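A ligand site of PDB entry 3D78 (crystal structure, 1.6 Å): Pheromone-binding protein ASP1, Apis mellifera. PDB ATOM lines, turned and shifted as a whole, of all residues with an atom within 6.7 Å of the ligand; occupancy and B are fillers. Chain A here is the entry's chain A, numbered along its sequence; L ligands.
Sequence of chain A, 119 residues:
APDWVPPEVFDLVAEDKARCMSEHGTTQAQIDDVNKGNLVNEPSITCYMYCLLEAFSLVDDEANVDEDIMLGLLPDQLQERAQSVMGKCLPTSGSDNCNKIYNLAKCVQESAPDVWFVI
A nitrogen (N1) of the ligand is in hydrogen-bond range of the backbone carbonyl oxygen of Phe 117, 2.8 Å away. An oxygen (O1) of the ligand is in hydrogen-bond range of the backbone NH (N) of Ile 119.
The side-chain sulfur (SD) of Met 49 is in hydrogen-bond range of the indole nitrogen (NE1) of Trp 116, at 3.6 Å. The chain-end carboxylate of Ile 119 sits at hydrogen-bond distance from the side-chain hydroxyl of Tyr 48 (2.6 Å). O of Leu 53 sits at hydrogen-bond distance from N of Leu 58 (2.9 Å).
The backbone carbonyl oxygen of Met 49 sits close to an oxygen (O2) of the ligand. CB of Leu 52 touches C6 of the ligand, at 3.7 Å. Leu 53 touches the ligand (CD2 to C6, 3.9 Å). CD1 of Leu 58 touches C7 of the ligand, 3.9 Å away. Val 115 touches the ligand. CE3 of Trp 116 touches C4 of the ligand, at 3.5 Å. Val 118 touches the ligand. Hydrophobic or aromatic side chains within 4 Å of the ligand: Met 49, Leu 52, Leu 53, Leu 58, Trp 116, Val 118 and Ile 119. Nine residues have an atom within 4 Å of the ligand: Met 49, Leu 52, Leu 53, Leu 58, Val 115, Trp 116, Phe 117, Val 118 and Ile 119. The nearest printed residue that does not touch the ligand is Val 13 (4.3 Å).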
ATOM      1  N   TRP A   4      33.229 -14.653  22.968  1.00  0.00           N
ATOM      2  CA  TRP A   4      32.325 -15.348  22.045  1.00  0.00           C
ATOM      3  C   TRP A   4      31.787 -14.460  20.935  1.00  0.00           C
ATOM      4  O   TRP A   4      31.218 -14.952  19.995  1.00  0.00           O
ATOM      5  CB  TRP A   4      31.153 -15.979  22.781  1.00  0.00           C
ATOM      6  CG  TRP A   4      30.282 -15.041  23.536  1.00  0.00           C
ATOM      7  CD1 TRP A   4      30.331 -14.811  24.863  1.00  0.00           C
ATOM      8  CD2 TRP A   4      29.173 -14.231  23.044  1.00  0.00           C
ATOM      9  NE1 TRP A   4      29.370 -13.913  25.234  1.00  0.00           N
ATOM     10  CE2 TRP A   4      28.657 -13.538  24.126  1.00  0.00           C
ATOM     11  CE3 TRP A   4      28.609 -14.017  21.784  1.00  0.00           C
ATOM     12  CZ2 TRP A   4      27.580 -12.668  24.005  1.00  0.00           C
ATOM     13  CZ3 TRP A   4      27.541 -13.135  21.677  1.00  0.00           C
ATOM     14  CH2 TRP A   4      27.035 -12.495  22.769  1.00  0.00           C
ATOM     15  N   VAL A   9      30.686  -8.719  13.975  1.00  0.00           N
ATOM     16  CA  VAL A   9      29.805  -7.733  14.653  1.00  0.00           C
ATOM     17  C   VAL A   9      30.508  -6.377  14.859  1.00  0.00           C
ATOM     18  O   VAL A   9      29.898  -5.298  14.768  1.00  0.00           O
ATOM     19  CB  VAL A   9      29.218  -8.313  15.978  1.00  0.00           C
ATOM     20  CG1 VAL A   9      28.360  -7.278  16.702  1.00  0.00           C
ATOM     21  CG2 VAL A   9      28.387  -9.576  15.682  1.00  0.00           C
ATOM     22  N   VAL A  13      28.569  -3.099  13.236  1.00  0.00           N
ATOM     23  CA  VAL A  13      28.055  -2.028  14.103  1.00  0.00           C
ATOM     24  C   VAL A  13      28.760  -0.698  13.961  1.00  0.00           C
ATOM     25  O   VAL A  13      28.323   0.295  14.536  1.00  0.00           O
ATOM     26  CB  VAL A  13      28.073  -2.428  15.615  1.00  0.00           C
ATOM     27  CG1 VAL A  13      27.320  -3.772  15.824  1.00  0.00           C
ATOM     28  CG2 VAL A  13      29.483  -2.416  16.177  1.00  0.00           C
ATOM     29  N   ILE A  31      31.274   2.924  27.749  1.00  0.00           N
ATOM     30  CA  ILE A  31      30.985   1.655  27.093  1.00  0.00           C
ATOM     31  C   ILE A  31      31.836   0.581  27.723  1.00  0.00           C
ATOM     32  O   ILE A  31      31.351  -0.502  28.031  1.00  0.00           O
ATOM     33  CB  ILE A  31      31.290   1.750  25.620  1.00  0.00           C
ATOM     34  CG1 ILE A  31      30.259   2.631  24.941  1.00  0.00           C
ATOM     35  CG2 ILE A  31      31.262   0.367  24.981  1.00  0.00           C
ATOM     36  CD1 ILE A  31      30.544   2.851  23.490  1.00  0.00           C
ATOM     37  N   TYR A  48      22.114   5.217  24.363  1.00  0.00           N
ATOM     38  CA  TYR A  48      23.077   4.666  23.392  1.00  0.00           C
ATOM     39  C   TYR A  48      22.782   3.194  23.092  1.00  0.00           C
ATOM     40  O   TYR A  48      22.739   2.788  21.935  1.00  0.00           O
ATOM     41  CB  TYR A  48      24.520   4.809  23.912  1.00  0.00           C
ATOM     42  CG  TYR A  48      25.511   4.094  23.046  1.00  0.00           C
ATOM     43  CD1 TYR A  48      25.868   4.610  21.806  1.00  0.00           C
ATOM     44  CD2 TYR A  48      26.078   2.885  23.426  1.00  0.00           C
ATOM     45  CE1 TYR A  48      26.793   3.959  20.981  1.00  0.00           C
ATOM     46  CE2 TYR A  48      26.976   2.226  22.595  1.00  0.00           C
ATOM     47  CZ  TYR A  48      27.332   2.765  21.379  1.00  0.00           C
ATOM     48  OH  TYR A  48      28.223   2.142  20.522  1.00  0.00           O
ATOM     49  N   MET A  49      22.602   2.386  24.133  1.00  0.00           N
ATOM     50  CA  MET A  49      22.209   0.991  23.952  1.00  0.00           C
ATOM     51  C   MET A  49      20.902   0.867  23.184  1.00  0.00           C
ATOM     52  O   MET A  49      20.776   0.085  22.257  1.00  0.00           O
ATOM     53  CB  MET A  49      22.112   0.315  25.304  1.00  0.00           C
ATOM     54  CG  MET A  49      23.481   0.118  25.949  1.00  0.00           C
ATOM     55  SD  MET A  49      23.468  -0.973  27.398  1.00  0.00           S
ATOM     56  CE  MET A  49      22.620   0.106  28.491  1.00  0.00           C
ATOM     57  N   TYR A  50      19.920   1.670  23.574  1.00  0.00           N
ATOM     58  CA  TYR A  50      18.652   1.659  22.831  1.00  0.00           C
ATOM     59  C   TYR A  50      18.928   1.946  21.345  1.00  0.00           C
ATOM     60  O   TYR A  50      18.420   1.261  20.457  1.00  0.00           O
ATOM     61  CB  TYR A  50      17.642   2.682  23.382  1.00  0.00           C
ATOM     62  CG  TYR A  50      16.429   2.772  22.467  1.00  0.00           C
ATOM     63  CD1 TYR A  50      15.429   1.835  22.523  1.00  0.00           C
ATOM     64  CD2 TYR A  50      16.370   3.709  21.442  1.00  0.00           C
ATOM     65  CE1 TYR A  50      14.334   1.877  21.638  1.00  0.00           C
ATOM     66  CE2 TYR A  50      15.297   3.734  20.544  1.00  0.00           C
ATOM     67  CZ  TYR A  50      14.280   2.839  20.660  1.00  0.00           C
ATOM     68  OH  TYR A  50      13.211   2.859  19.749  1.00  0.00           O
ATOM     69  N   CYS A  51      19.698   3.011  21.087  1.00  0.00           N
ATOM     70  CA  CYS A  51      20.036   3.456  19.718  1.00  0.00           C
ATOM     71  C   CYS A  51      20.659   2.314  18.877  1.00  0.00           C
ATOM     72  O   CYS A  51      20.273   2.077  17.719  1.00  0.00           O
ATOM     73  CB  CYS A  51      21.021   4.635  19.797  1.00  0.00           C
ATOM     74  SG  CYS A  51      21.388   5.482  18.221  1.00  0.00           S
ATOM     75  N   LEU A  52      21.590   1.586  19.473  1.00  0.00           N
ATOM     76  CA  LEU A  52      22.320   0.578  18.715  1.00  0.00           C
ATOM     77  C   LEU A  52      21.375  -0.616  18.485  1.00  0.00           C
ATOM     78  O   LEU A  52      21.315  -1.200  17.386  1.00  0.00           O
ATOM     79  CB  LEU A  52      23.616   0.192  19.445  1.00  0.00           C
ATOM     80  CG  LEU A  52      24.770  -0.326  18.607  1.00  0.00           C
ATOM     81  CD1 LEU A  52      25.069   0.527  17.404  1.00  0.00           C
ATOM     82  CD2 LEU A  52      26.008  -0.516  19.547  1.00  0.00           C
ATOM     83  N   LEU A  53      20.598  -0.976  19.495  1.00  0.00           N
ATOM     84  CA  LEU A  53      19.619  -2.055  19.344  1.00  0.00           C
ATOM     85  C   LEU A  53      18.624  -1.713  18.238  1.00  0.00           C
ATOM     86  O   LEU A  53      18.307  -2.537  17.386  1.00  0.00           O
ATOM     87  CB  LEU A  53      18.870  -2.315  20.652  1.00  0.00           C
ATOM     88  CG  LEU A  53      19.688  -2.985  21.747  1.00  0.00           C
ATOM     89  CD1 LEU A  53      18.921  -2.815  23.093  1.00  0.00           C
ATOM     90  CD2 LEU A  53      20.018  -4.449  21.452  1.00  0.00           C
ATOM     91  N   GLU A  54      18.119  -0.501  18.259  1.00  0.00           N
ATOM     92  CA  GLU A  54      17.126  -0.075  17.282  1.00  0.00           C
ATOM     93  C   GLU A  54      17.693  -0.112  15.870  1.00  0.00           C
ATOM     94  O   GLU A  54      17.011  -0.480  14.918  1.00  0.00           O
ATOM     95  CB  GLU A  54      16.587   1.313  17.602  1.00  0.00           C
ATOM     96  CG  GLU A  54      15.316   1.684  16.800  1.00  0.00           C
ATOM     97  CD  GLU A  54      15.560   2.036  15.363  1.00  0.00           C
ATOM     98  OE1 GLU A  54      16.656   2.545  15.041  1.00  0.00           O
ATOM     99  OE2 GLU A  54      14.626   1.817  14.546  1.00  0.00           O
ATOM    100  N   PHE A  56      19.574  -2.208  14.548  1.00  0.00           N
ATOM    101  CA  PHE A  56      19.551  -3.567  14.070  1.00  0.00           C
ATOM    102  C   PHE A  56      18.194  -4.236  14.192  1.00  0.00           C
ATOM    103  O   PHE A  56      18.086  -5.458  14.003  1.00  0.00           O
ATOM    104  CB  PHE A  56      20.667  -4.310  14.758  1.00  0.00           C
ATOM    105  CG  PHE A  56      21.995  -3.886  14.217  1.00  0.00           C
ATOM    106  CD1 PHE A  56      22.352  -4.242  12.919  1.00  0.00           C
ATOM    107  CD2 PHE A  56      22.776  -3.002  14.912  1.00  0.00           C
ATOM    108  CE1 PHE A  56      23.526  -3.807  12.373  1.00  0.00           C
ATOM    109  CE2 PHE A  56      23.972  -2.552  14.368  1.00  0.00           C
ATOM    110  CZ  PHE A  56      24.340  -2.938  13.103  1.00  0.00           C
ATOM    111  N   LEU A  58      16.570  -4.801  16.719  1.00  0.00           N
ATOM    112  CA  LEU A  58      16.493  -5.719  17.877  1.00  0.00           C
ATOM    113  C   LEU A  58      15.406  -5.299  18.858  1.00  0.00           C
ATOM    114  O   LEU A  58      14.890  -6.117  19.631  1.00  0.00           O
ATOM    115  CB  LEU A  58      17.856  -5.815  18.584  1.00  0.00           C
ATOM    116  CG  LEU A  58      18.958  -6.469  17.746  1.00  0.00           C
ATOM    117  CD1 LEU A  58      20.350  -6.095  18.288  1.00  0.00           C
ATOM    118  CD2 LEU A  58      18.795  -7.950  17.718  1.00  0.00           C
ATOM    119  N   MET A  70      16.966 -11.088  17.672  1.00  0.00           N
ATOM    120  CA  MET A  70      18.042 -11.237  18.657  1.00  0.00           C
ATOM    121  C   MET A  70      18.707 -12.602  18.515  1.00  0.00           C
ATOM    122  O   MET A  70      19.934 -12.704  18.438  1.00  0.00           O
ATOM    123  CB  MET A  70      17.500 -11.039  20.077  1.00  0.00           C
ATOM    124  CG  MET A  70      18.516 -11.291  21.210  1.00  0.00           C
ATOM    125  SD  MET A  70      19.739  -9.990  21.350  1.00  0.00           S
ATOM    126  CE  MET A  70      18.834  -8.647  22.115  1.00  0.00           C
ATOM    127  N   LEU A  73      20.947 -12.930  15.426  1.00  0.00           N
ATOM    128  CA  LEU A  73      22.227 -12.228  15.433  1.00  0.00           C
ATOM    129  C   LEU A  73      23.229 -12.973  16.287  1.00  0.00           C
ATOM    130  O   LEU A  73      24.412 -12.998  15.989  1.00  0.00           O
ATOM    131  CB  LEU A  73      22.057 -10.778  15.918  1.00  0.00           C
ATOM    132  CG  LEU A  73      23.289  -9.874  15.729  1.00  0.00           C
ATOM    133  CD1 LEU A  73      23.637  -9.789  14.256  1.00  0.00           C
ATOM    134  CD2 LEU A  73      23.084  -8.481  16.281  1.00  0.00           C
ATOM    135  N   LEU A  74      22.735 -13.594  17.353  1.00  0.00           N
ATOM    136  CA  LEU A  74      23.573 -14.337  18.284  1.00  0.00           C
ATOM    137  C   LEU A  74      24.102 -15.615  17.651  1.00  0.00           C
ATOM    138  O   LEU A  74      23.418 -16.268  16.866  1.00  0.00           O
ATOM    139  CB  LEU A  74      22.781 -14.679  19.557  1.00  0.00           C
ATOM    140  CG  LEU A  74      22.487 -13.524  20.512  1.00  0.00           C
ATOM    141  CD1 LEU A  74      21.517 -13.950  21.602  1.00  0.00           C
ATOM    142  CD2 LEU A  74      23.748 -12.964  21.173  1.00  0.00           C
ATOM    143  N   ILE A 101      15.700  -0.365  28.485  1.00  0.00           N
ATOM    144  CA  ILE A 101      16.936  -1.051  28.123  1.00  0.00           C
ATOM    145  C   ILE A 101      17.860  -1.185  29.366  1.00  0.00           C
ATOM    146  O   ILE A 101      18.491  -2.235  29.606  1.00  0.00           O
ATOM    147  CB  ILE A 101      17.616  -0.374  26.933  1.00  0.00           C
ATOM    148  CG1 ILE A 101      16.685  -0.404  25.702  1.00  0.00           C
ATOM    149  CG2 ILE A 101      18.973  -1.047  26.675  1.00  0.00           C
ATOM    150  CD1 ILE A 101      16.062  -1.783  25.327  1.00  0.00           C
ATOM    151  N   VAL A 108      19.605  -9.131  32.738  1.00  0.00           N
ATOM    152  CA  VAL A 108      20.478 -10.106  32.069  1.00  0.00           C
ATOM    153  C   VAL A 108      21.722 -10.280  32.894  1.00  0.00           C
ATOM    154  O   VAL A 108      22.189 -11.406  33.149  1.00  0.00           O
ATOM    155  CB  VAL A 108      20.794  -9.718  30.604  1.00  0.00           C
ATOM    156  CG1 VAL A 108      21.753 -10.724  29.997  1.00  0.00           C
ATOM    157  CG2 VAL A 108      19.522  -9.665  29.782  1.00  0.00           C
ATOM    158  N   VAL A 115      26.422 -12.584  28.748  1.00  0.00           N
ATOM    159  CA  VAL A 115      25.548 -12.630  27.598  1.00  0.00           C
ATOM    160  C   VAL A 115      25.282 -11.205  27.081  1.00  0.00           C
ATOM    161  O   VAL A 115      25.005 -11.014  25.889  1.00  0.00           O
ATOM    162  CB  VAL A 115      24.239 -13.398  27.888  1.00  0.00           C
ATOM    163  CG1 VAL A 115      23.180 -13.159  26.762  1.00  0.00           C
ATOM    164  CG2 VAL A 115      24.555 -14.896  28.083  1.00  0.00           C
ATOM    165  N   TRP A 116      25.276 -10.221  27.970  1.00  0.00           N
ATOM    166  CA  TRP A 116      25.069  -8.793  27.657  1.00  0.00           C
ATOM    167  C   TRP A 116      26.428  -8.155  27.460  1.00  0.00           C
ATOM    168  O   TRP A 116      27.382  -8.485  28.197  1.00  0.00           O
ATOM    169  CB  TRP A 116      24.348  -8.050  28.814  1.00  0.00           C
ATOM    170  CG  TRP A 116      23.863  -6.681  28.383  1.00  0.00           C
ATOM    171  CD1 TRP A 116      24.539  -5.496  28.476  1.00  0.00           C
ATOM    172  CD2 TRP A 116      22.641  -6.408  27.719  1.00  0.00           C
ATOM    173  NE1 TRP A 116      23.774  -4.480  27.930  1.00  0.00           N
ATOM    174  CE2 TRP A 116      22.607  -5.022  27.455  1.00  0.00           C
ATOM    175  CE3 TRP A 116      21.557  -7.186  27.308  1.00  0.00           C
ATOM    176  CZ2 TRP A 116      21.543  -4.408  26.802  1.00  0.00           C
ATOM    177  CZ3 TRP A 116      20.505  -6.582  26.698  1.00  0.00           C
ATOM    178  CH2 TRP A 116      20.505  -5.205  26.423  1.00  0.00           C
ATOM    179  N   PHE A 117      26.564  -7.267  26.492  1.00  0.00           N
ATOM    180  CA  PHE A 117      27.772  -6.483  26.360  1.00  0.00           C
ATOM    181  C   PHE A 117      27.375  -5.250  25.580  1.00  0.00           C
ATOM    182  O   PHE A 117      26.325  -5.215  24.958  1.00  0.00           O
ATOM    183  CB  PHE A 117      28.892  -7.226  25.641  1.00  0.00           C
ATOM    184  CG  PHE A 117      28.590  -7.540  24.216  1.00  0.00           C
ATOM    185  CD1 PHE A 117      27.798  -8.619  23.874  1.00  0.00           C
ATOM    186  CD2 PHE A 117      29.073  -6.735  23.204  1.00  0.00           C
ATOM    187  CE1 PHE A 117      27.470  -8.857  22.543  1.00  0.00           C
ATOM    188  CE2 PHE A 117      28.790  -7.002  21.885  1.00  0.00           C
ATOM    189  CZ  PHE A 117      27.983  -8.048  21.553  1.00  0.00           C
ATOM    190  N   VAL A 118      28.235  -4.263  25.647  1.00  0.00           N
ATOM    191  CA  VAL A 118      28.070  -3.021  24.912  1.00  0.00           C
ATOM    192  C   VAL A 118      29.301  -2.844  24.050  1.00  0.00           C
ATOM    193  O   VAL A 118      30.450  -3.129  24.425  1.00  0.00           O
ATOM    194  CB  VAL A 118      27.834  -1.821  25.825  1.00  0.00           C
ATOM    195  CG1 VAL A 118      27.656  -0.514  25.000  1.00  0.00           C
ATOM    196  CG2 VAL A 118      26.600  -2.045  26.700  1.00  0.00           C
ATOM    197  N   ILE A 119      29.041  -2.391  22.844  1.00  0.00           N
ATOM    198  CA  ILE A 119      30.069  -2.208  21.866  1.00  0.00           C
ATOM    199  C   ILE A 119      30.087  -0.755  21.447  1.00  0.00           C
ATOM    200  O   ILE A 119      31.107  -0.194  21.068  1.00  0.00           O
ATOM    201  CB  ILE A 119      29.759  -3.076  20.649  1.00  0.00           C
ATOM    202  CG1 ILE A 119      30.831  -2.898  19.593  1.00  0.00           C
ATOM    203  CG2 ILE A 119      28.348  -2.757  20.111  1.00  0.00           C
ATOM    204  CD1 ILE A 119      32.264  -3.011  20.104  1.00  0.00           C
ATOM    205  OXT ILE A 119      29.018  -0.159  21.478  1.00  0.00           O
HETATM  206  O1  LIG L   1      25.600  -2.309  23.078  1.00  0.00           O
HETATM  207  S1  LIG L   1      24.317  -2.955  22.828  1.00  0.00           S
HETATM  208  O2  LIG L   1      23.351  -1.796  22.787  1.00  0.00           O
HETATM  209  N1  LIG L   1      23.969  -4.102  23.848  1.00  0.00           N
HETATM  210  C1  LIG L   1      23.246  -5.408  23.555  1.00  0.00           C
HETATM  211  C2  LIG L   1      23.618  -6.695  24.365  1.00  0.00           C
HETATM  212  C3  LIG L   1      23.199  -8.087  23.829  1.00  0.00           C
HETATM  213  C4  LIG L   1      22.778  -9.209  24.784  1.00  0.00           C
HETATM  214  C5  LIG L   1      24.421  -3.699  21.386  1.00  0.00           C
HETATM  215  C6  LIG L   1      23.564  -3.400  20.350  1.00  0.00           C
HETATM  216  C7  LIG L   1      23.607  -4.018  19.107  1.00  0.00           C
HETATM  217  C8  LIG L   1      24.555  -4.991  18.905  1.00  0.00           C
HETATM  218  C9  LIG L   1      25.413  -5.341  19.939  1.00  0.00           C
HETATM  219  C10 LIG L   1      25.363  -4.701  21.182  1.00  0.00           C
